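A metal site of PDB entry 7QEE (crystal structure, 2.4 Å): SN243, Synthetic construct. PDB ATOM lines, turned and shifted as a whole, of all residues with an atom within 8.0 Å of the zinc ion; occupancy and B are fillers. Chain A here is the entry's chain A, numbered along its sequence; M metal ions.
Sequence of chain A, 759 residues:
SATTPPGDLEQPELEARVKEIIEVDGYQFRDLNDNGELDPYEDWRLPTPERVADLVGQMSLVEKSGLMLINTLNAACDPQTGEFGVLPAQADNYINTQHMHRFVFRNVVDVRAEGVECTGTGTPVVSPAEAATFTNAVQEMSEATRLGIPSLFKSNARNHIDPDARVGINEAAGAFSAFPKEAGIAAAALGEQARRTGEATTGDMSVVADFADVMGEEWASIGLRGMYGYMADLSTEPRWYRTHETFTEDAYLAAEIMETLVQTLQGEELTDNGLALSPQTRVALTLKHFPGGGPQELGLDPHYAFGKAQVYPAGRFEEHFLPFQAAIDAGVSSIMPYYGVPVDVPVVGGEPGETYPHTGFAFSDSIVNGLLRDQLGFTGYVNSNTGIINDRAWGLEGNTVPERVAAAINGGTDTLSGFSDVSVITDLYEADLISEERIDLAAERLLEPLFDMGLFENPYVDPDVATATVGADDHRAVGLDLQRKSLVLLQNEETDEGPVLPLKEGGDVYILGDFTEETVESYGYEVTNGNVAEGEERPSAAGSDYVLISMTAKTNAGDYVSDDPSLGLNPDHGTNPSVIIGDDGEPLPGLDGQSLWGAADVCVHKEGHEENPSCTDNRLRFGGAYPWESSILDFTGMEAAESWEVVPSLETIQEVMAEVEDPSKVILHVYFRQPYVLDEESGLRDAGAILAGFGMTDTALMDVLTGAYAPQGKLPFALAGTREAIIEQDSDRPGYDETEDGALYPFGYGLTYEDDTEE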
ATOM      1  N   GLU A  20     -17.934 -20.159   3.604  1.00  0.00           N
ATOM      2  CA  GLU A  20     -16.706 -20.647   4.205  1.00  0.00           C
ATOM      3  C   GLU A  20     -17.009 -21.706   5.258  1.00  0.00           C
ATOM      4  O   GLU A  20     -18.080 -21.707   5.859  1.00  0.00           O
ATOM      5  CB  GLU A  20     -15.918 -19.490   4.850  1.00  0.00           C
ATOM      6  CG  GLU A  20     -14.813 -18.855   3.982  1.00  0.00           C
ATOM      7  CD  GLU A  20     -15.250 -17.547   3.302  1.00  0.00           C
ATOM      8  OE1 GLU A  20     -16.366 -17.053   3.588  1.00  0.00           O
ATOM      9  OE2 GLU A  20     -14.466 -17.007   2.497  1.00  0.00           O
ATOM     10  N   ILE A  22     -15.970 -23.483   8.984  1.00  0.00           N
ATOM     11  CA  ILE A  22     -15.396 -22.979  10.214  1.00  0.00           C
ATOM     12  C   ILE A  22     -15.259 -24.117  11.215  1.00  0.00           C
ATOM     13  O   ILE A  22     -16.133 -24.995  11.321  1.00  0.00           O
ATOM     14  CB  ILE A  22     -16.169 -21.819  10.867  1.00  0.00           C
ATOM     15  CG1 ILE A  22     -17.532 -22.283  11.392  1.00  0.00           C
ATOM     16  CG2 ILE A  22     -16.208 -20.629   9.932  1.00  0.00           C
ATOM     17  CD1 ILE A  22     -18.461 -21.150  11.784  1.00  0.00           C
ATOM     18  N   PHE A  29     -17.943 -27.167  10.272  1.00  0.00           N
ATOM     19  CA  PHE A  29     -19.291 -26.650  10.077  1.00  0.00           C
ATOM     20  C   PHE A  29     -19.263 -25.637   8.942  1.00  0.00           C
ATOM     21  O   PHE A  29     -18.242 -24.995   8.705  1.00  0.00           O
ATOM     22  CB  PHE A  29     -19.829 -25.963  11.351  1.00  0.00           C
ATOM     23  CG  PHE A  29     -19.807 -26.842  12.587  1.00  0.00           C
ATOM     24  CD1 PHE A  29     -20.875 -27.693  12.876  1.00  0.00           C
ATOM     25  CD2 PHE A  29     -18.734 -26.811  13.459  1.00  0.00           C
ATOM     26  CE1 PHE A  29     -20.855 -28.504  14.010  1.00  0.00           C
ATOM     27  CE2 PHE A  29     -18.714 -27.614  14.600  1.00  0.00           C
ATOM     28  CZ  PHE A  29     -19.774 -28.462  14.884  1.00  0.00           C
ATOM     29  N   ARG A  30     -20.401 -25.474   8.266  1.00  0.00           N
ATOM     30  CA  ARG A  30     -20.531 -24.481   7.198  1.00  0.00           C
ATOM     31  C   ARG A  30     -21.100 -23.169   7.726  1.00  0.00           C
ATOM     32  O   ARG A  30     -22.155 -23.159   8.358  1.00  0.00           O
ATOM     33  CB  ARG A  30     -21.409 -24.990   6.067  1.00  0.00           C
ATOM     34  CG  ARG A  30     -20.776 -26.111   5.286  1.00  0.00           C
ATOM     35  CD  ARG A  30     -21.785 -26.844   4.420  1.00  0.00           C
ATOM     36  NE  ARG A  30     -22.006 -26.191   3.124  1.00  0.00           N
ATOM     37  CZ  ARG A  30     -23.183 -26.166   2.511  1.00  0.00           C
ATOM     38  NH1 ARG A  30     -23.315 -25.567   1.335  1.00  0.00           N
ATOM     39  NH2 ARG A  30     -24.223 -26.754   3.088  1.00  0.00           N
ATOM     40  N   ASP A  31     -20.413 -22.060   7.426  1.00  0.00           N
ATOM     41  CA  ASP A  31     -20.819 -20.734   7.892  1.00  0.00           C
ATOM     42  C   ASP A  31     -21.776 -20.101   6.874  1.00  0.00           C
ATOM     43  O   ASP A  31     -21.440 -19.186   6.115  1.00  0.00           O
ATOM     44  CB  ASP A  31     -19.592 -19.857   8.113  1.00  0.00           C
ATOM     45  CG  ASP A  31     -19.947 -18.416   8.437  1.00  0.00           C
ATOM     46  OD1 ASP A  31     -20.840 -18.218   9.276  1.00  0.00           O
ATOM     47  OD2 ASP A  31     -19.330 -17.490   7.855  1.00  0.00           O
ATOM     48  N   LEU A  32     -23.016 -20.616   6.884  1.00  0.00           N
ATOM     49  CA  LEU A  32     -23.951 -20.356   5.790  1.00  0.00           C
ATOM     50  C   LEU A  32     -24.496 -18.935   5.791  1.00  0.00           C
ATOM     51  O   LEU A  32     -25.000 -18.467   4.767  1.00  0.00           O
ATOM     52  CB  LEU A  32     -25.094 -21.374   5.841  1.00  0.00           C
ATOM     53  CG  LEU A  32     -24.768 -22.786   5.328  1.00  0.00           C
ATOM     54  CD1 LEU A  32     -25.781 -23.761   5.846  1.00  0.00           C
ATOM     55  CD2 LEU A  32     -24.770 -22.808   3.804  1.00  0.00           C
ATOM     56  N   ASN A  33     -24.483 -18.257   6.941  1.00  0.00           N
ATOM     57  CA  ASN A  33     -24.894 -16.865   7.031  1.00  0.00           C
ATOM     58  C   ASN A  33     -23.736 -15.892   6.852  1.00  0.00           C
ATOM     59  O   ASN A  33     -23.958 -14.678   6.934  1.00  0.00           O
ATOM     60  CB  ASN A  33     -25.570 -16.613   8.373  1.00  0.00           C
ATOM     61  CG  ASN A  33     -24.651 -16.908   9.549  1.00  0.00           C
ATOM     62  OD1 ASN A  33     -23.447 -17.150   9.381  1.00  0.00           O
ATOM     63  ND2 ASN A  33     -25.225 -16.919  10.749  1.00  0.00           N
ATOM     64  N   ASP A  34     -22.499 -16.399   6.669  1.00  0.00           N
ATOM     65  CA  ASP A  34     -21.320 -15.577   6.399  1.00  0.00           C
ATOM     66  C   ASP A  34     -21.046 -14.613   7.553  1.00  0.00           C
ATOM     67  O   ASP A  34     -20.571 -13.498   7.342  1.00  0.00           O
ATOM     68  CB  ASP A  34     -21.410 -14.805   5.078  1.00  0.00           C
ATOM     69  CG  ASP A  34     -20.017 -14.475   4.488  1.00  0.00           C
ATOM     70  OD1 ASP A  34     -19.028 -15.134   4.902  1.00  0.00           O
ATOM     71  OD2 ASP A  34     -19.909 -13.559   3.637  1.00  0.00           O
ATOM     72  N   ASN A  35     -21.435 -15.004   8.770  1.00  0.00           N
ATOM     73  CA  ASN A  35     -21.213 -14.152   9.932  1.00  0.00           C
ATOM     74  C   ASN A  35     -19.974 -14.544  10.722  1.00  0.00           C
ATOM     75  O   ASN A  35     -19.744 -13.966  11.794  1.00  0.00           O
ATOM     76  CB  ASN A  35     -22.450 -14.137  10.827  1.00  0.00           C
ATOM     77  CG  ASN A  35     -22.588 -15.387  11.655  1.00  0.00           C
ATOM     78  OD1 ASN A  35     -21.868 -16.347  11.468  1.00  0.00           O
ATOM     79  ND2 ASN A  35     -23.511 -15.369  12.615  1.00  0.00           N
ATOM     80  N   GLY A  36     -19.218 -15.529  10.280  1.00  0.00           N
ATOM     81  CA  GLY A  36     -17.984 -15.881  10.941  1.00  0.00           C
ATOM     82  C   GLY A  36     -18.113 -16.700  12.203  1.00  0.00           C
ATOM     83  O   GLY A  36     -17.118 -17.296  12.637  1.00  0.00           O
ATOM     84  N   GLU A  37     -19.278 -16.717  12.831  1.00  0.00           N
ATOM     85  CA  GLU A  37     -19.498 -17.593  13.974  1.00  0.00           C
ATOM     86  C   GLU A  37     -20.544 -18.652  13.634  1.00  0.00           C
ATOM     87  O   GLU A  37     -21.280 -18.558  12.651  1.00  0.00           O
ATOM     88  CB  GLU A  37     -19.869 -16.784  15.218  1.00  0.00           C
ATOM     89  CG  GLU A  37     -18.914 -15.609  15.446  1.00  0.00           C
ATOM     90  CD  GLU A  37     -17.845 -15.882  16.509  1.00  0.00           C
ATOM     91  OE1 GLU A  37     -16.896 -15.072  16.627  1.00  0.00           O
ATOM     92  OE2 GLU A  37     -17.930 -16.915  17.204  1.00  0.00           O
ATOM     93  N   LEU A  38     -20.613 -19.689  14.462  1.00  0.00           N
ATOM     94  CA  LEU A  38     -21.461 -20.847  14.190  1.00  0.00           C
ATOM     95  C   LEU A  38     -22.835 -20.672  14.828  1.00  0.00           C
ATOM     96  O   LEU A  38     -22.956 -20.704  16.059  1.00  0.00           O
ATOM     97  CB  LEU A  38     -20.767 -22.112  14.695  1.00  0.00           C
ATOM     98  CG  LEU A  38     -21.632 -23.363  14.800  1.00  0.00           C
ATOM     99  CD1 LEU A  38     -21.867 -23.939  13.420  1.00  0.00           C
ATOM    100  CD2 LEU A  38     -20.983 -24.390  15.700  1.00  0.00           C
ATOM    101  N   ASP A  39     -23.880 -20.483  13.998  1.00  0.00           N
ATOM    102  CA  ASP A  39     -25.272 -20.472  14.461  1.00  0.00           C
ATOM    103  C   ASP A  39     -25.779 -21.875  14.761  1.00  0.00           C
ATOM    104  O   ASP A  39     -25.259 -22.873  14.242  1.00  0.00           O
ATOM    105  CB  ASP A  39     -26.185 -19.826  13.439  1.00  0.00           C
ATOM    106  CG  ASP A  39     -25.832 -18.398  13.172  1.00  0.00           C
ATOM    107  OD1 ASP A  39     -24.626 -18.094  13.097  1.00  0.00           O
ATOM    108  OD2 ASP A  39     -26.760 -17.573  13.014  1.00  0.00           O
ATOM    109  N   PRO A  40     -26.808 -21.993  15.614  1.00  0.00           N
ATOM    110  CA  PRO A  40     -27.430 -23.319  15.831  1.00  0.00           C
ATOM    111  C   PRO A  40     -27.895 -24.018  14.562  1.00  0.00           C
ATOM    112  O   PRO A  40     -27.781 -25.248  14.465  1.00  0.00           O
ATOM    113  CB  PRO A  40     -28.609 -22.991  16.752  1.00  0.00           C
ATOM    114  CG  PRO A  40     -28.183 -21.771  17.488  1.00  0.00           C
ATOM    115  CD  PRO A  40     -27.356 -20.967  16.516  1.00  0.00           C
ATOM    116  N   TYR A  41     -28.422 -23.268  13.577  1.00  0.00           N
ATOM    117  CA  TYR A  41     -28.930 -23.909  12.368  1.00  0.00           C
ATOM    118  C   TYR A  41     -27.813 -24.460  11.486  1.00  0.00           C
ATOM    119  O   TYR A  41     -28.055 -25.356  10.679  1.00  0.00           O
ATOM    120  CB  TYR A  41     -29.840 -22.950  11.600  1.00  0.00           C
ATOM    121  CG  TYR A  41     -29.204 -22.056  10.582  1.00  0.00           C
ATOM    122  CD1 TYR A  41     -29.088 -22.461   9.260  1.00  0.00           C
ATOM    123  CD2 TYR A  41     -28.792 -20.778  10.906  1.00  0.00           C
ATOM    124  CE1 TYR A  41     -28.529 -21.633   8.291  1.00  0.00           C
ATOM    125  CE2 TYR A  41     -28.224 -19.938   9.939  1.00  0.00           C
ATOM    126  CZ  TYR A  41     -28.104 -20.375   8.636  1.00  0.00           C
ATOM    127  OH  TYR A  41     -27.553 -19.558   7.665  1.00  0.00           O
ATOM    128  N   GLU A  42     -26.598 -23.921  11.613  1.00  0.00           N
ATOM    129  CA  GLU A  42     -25.428 -24.472  10.958  1.00  0.00           C
ATOM    130  C   GLU A  42     -24.782 -25.606  11.766  1.00  0.00           C
ATOM    131  O   GLU A  42     -23.815 -26.221  11.289  1.00  0.00           O
ATOM    132  CB  GLU A  42     -24.414 -23.359  10.705  1.00  0.00           C
ATOM    133  CG  GLU A  42     -24.980 -22.194   9.883  1.00  0.00           C
ATOM    134  CD  GLU A  42     -24.259 -20.878  10.177  1.00  0.00           C
ATOM    135  OE1 GLU A  42     -23.707 -20.756  11.302  1.00  0.00           O
ATOM    136  OE2 GLU A  42     -24.253 -19.982   9.300  1.00  0.00           O
ATOM    137  N   ASP A  43     -25.283 -25.896  12.962  1.00  0.00           N
ATOM    138  CA  ASP A  43     -24.661 -26.844  13.884  1.00  0.00           C
ATOM    139  C   ASP A  43     -25.320 -28.205  13.718  1.00  0.00           C
ATOM    140  O   ASP A  43     -26.319 -28.516  14.363  1.00  0.00           O
ATOM    141  CB  ASP A  43     -24.778 -26.322  15.316  1.00  0.00           C
ATOM    142  CG  ASP A  43     -24.049 -27.192  16.318  1.00  0.00           C
ATOM    143  OD1 ASP A  43     -24.058 -28.434  16.174  1.00  0.00           O
ATOM    144  OD2 ASP A  43     -23.446 -26.634  17.253  1.00  0.00           O
ATOM    145  N   ASP A  54     -33.923 -21.984  15.043  1.00  0.00           N
ATOM    146  CA  ASP A  54     -32.906 -20.937  14.933  1.00  0.00           C
ATOM    147  C   ASP A  54     -32.896 -20.313  13.539  1.00  0.00           C
ATOM    148  O   ASP A  54     -32.556 -19.126  13.384  1.00  0.00           O
ATOM    149  CB  ASP A  54     -31.530 -21.471  15.288  1.00  0.00           C
ATOM    150  CG  ASP A  54     -30.478 -20.376  15.283  1.00  0.00           C
ATOM    151  OD1 ASP A  54     -30.277 -19.720  16.319  1.00  0.00           O
ATOM    152  OD2 ASP A  54     -29.882 -20.138  14.220  1.00  0.00           O
ATOM    153  N   GLN A  58     -34.199 -16.072  11.994  1.00  0.00           N
ATOM    154  CA  GLN A  58     -33.376 -15.115  11.270  1.00  0.00           C
ATOM    155  C   GLN A  58     -33.909 -14.761   9.886  1.00  0.00           C
ATOM    156  O   GLN A  58     -33.186 -14.112   9.119  1.00  0.00           O
ATOM    157  CB  GLN A  58     -31.966 -15.673  11.121  1.00  0.00           C
ATOM    158  CG  GLN A  58     -31.417 -16.300  12.368  1.00  0.00           C
ATOM    159  CD  GLN A  58     -30.057 -16.921  12.117  1.00  0.00           C
ATOM    160  OE1 GLN A  58     -29.268 -16.403  11.320  1.00  0.00           O
ATOM    161  NE2 GLN A  58     -29.771 -18.018  12.809  1.00  0.00           N
HETATM  162 ZN    ZN M   1     -22.753 -18.834  11.132  1.00  0.00          ZN
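Merely in contact with the zinc ion: Leu 38 (3.9 Å). Within 4 Å of the zinc ion: Asp 31, Asn 33, Asn 35, Glu 37, Leu 38, Asp 39 and Glu 42.
The zinc ion is bound by the backbone carbonyl oxygen (O) of Glu 37 (2.1 Å), the side-chain carboxylate (OE1) of Glu 42 (2.2 Å) and the side-chain amide oxygen (OD1) of Asn 33 (2.5 Å). The zinc ion has three donor atoms within binding distance. Slightly farther from the zinc ion lies the side-chain carboxylate (OE2) of Glu 42 (2.6 Å). Slightly farther from the zinc ion lies OD1 of Asn 35 (2.7 Å). Slightly farther from the zinc ion lies the side-chain carboxylate (OD1) of Asp 31 (2.7 Å). Slightly farther from the zinc ion lies the side-chain carboxylate (OD1) of Asp 39 (2.8 Å).
OD1 of Asn 35 sits at hydrogen-bond distance from N of Glu 37, 3.0 Å away. The backbone NH (N) of Asp 39 sits close to the side-chain carboxylate (OE1) of Glu 42 (2.7 Å). ND2 of Asn 35 sits close to ND2 of Asn 33. The side-chain amide oxygen (OD1) of Asn 33 sits close to the side-chain carboxylate (OD1) of Asp 31, at 2.8 Å. The side-chain amide nitrogen (ND2) of Asn 33 is in hydrogen-bond range of the side-chain carboxylate (OD1) of Asp 39 (2.7 Å). The backbone NH (N) of Asn 33 lies within hydrogen-bond range of the side-chain hydroxyl (OH) of Tyr 41, at 3.4 Å. ND2 of Asn 35 sits at hydrogen-bond distance from OD1 of Asp 39. The side-chain carboxylate of Asp 39 sits at hydrogen-bond distance from the side-chain amide nitrogen of Gln 58 (3.1 Å).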
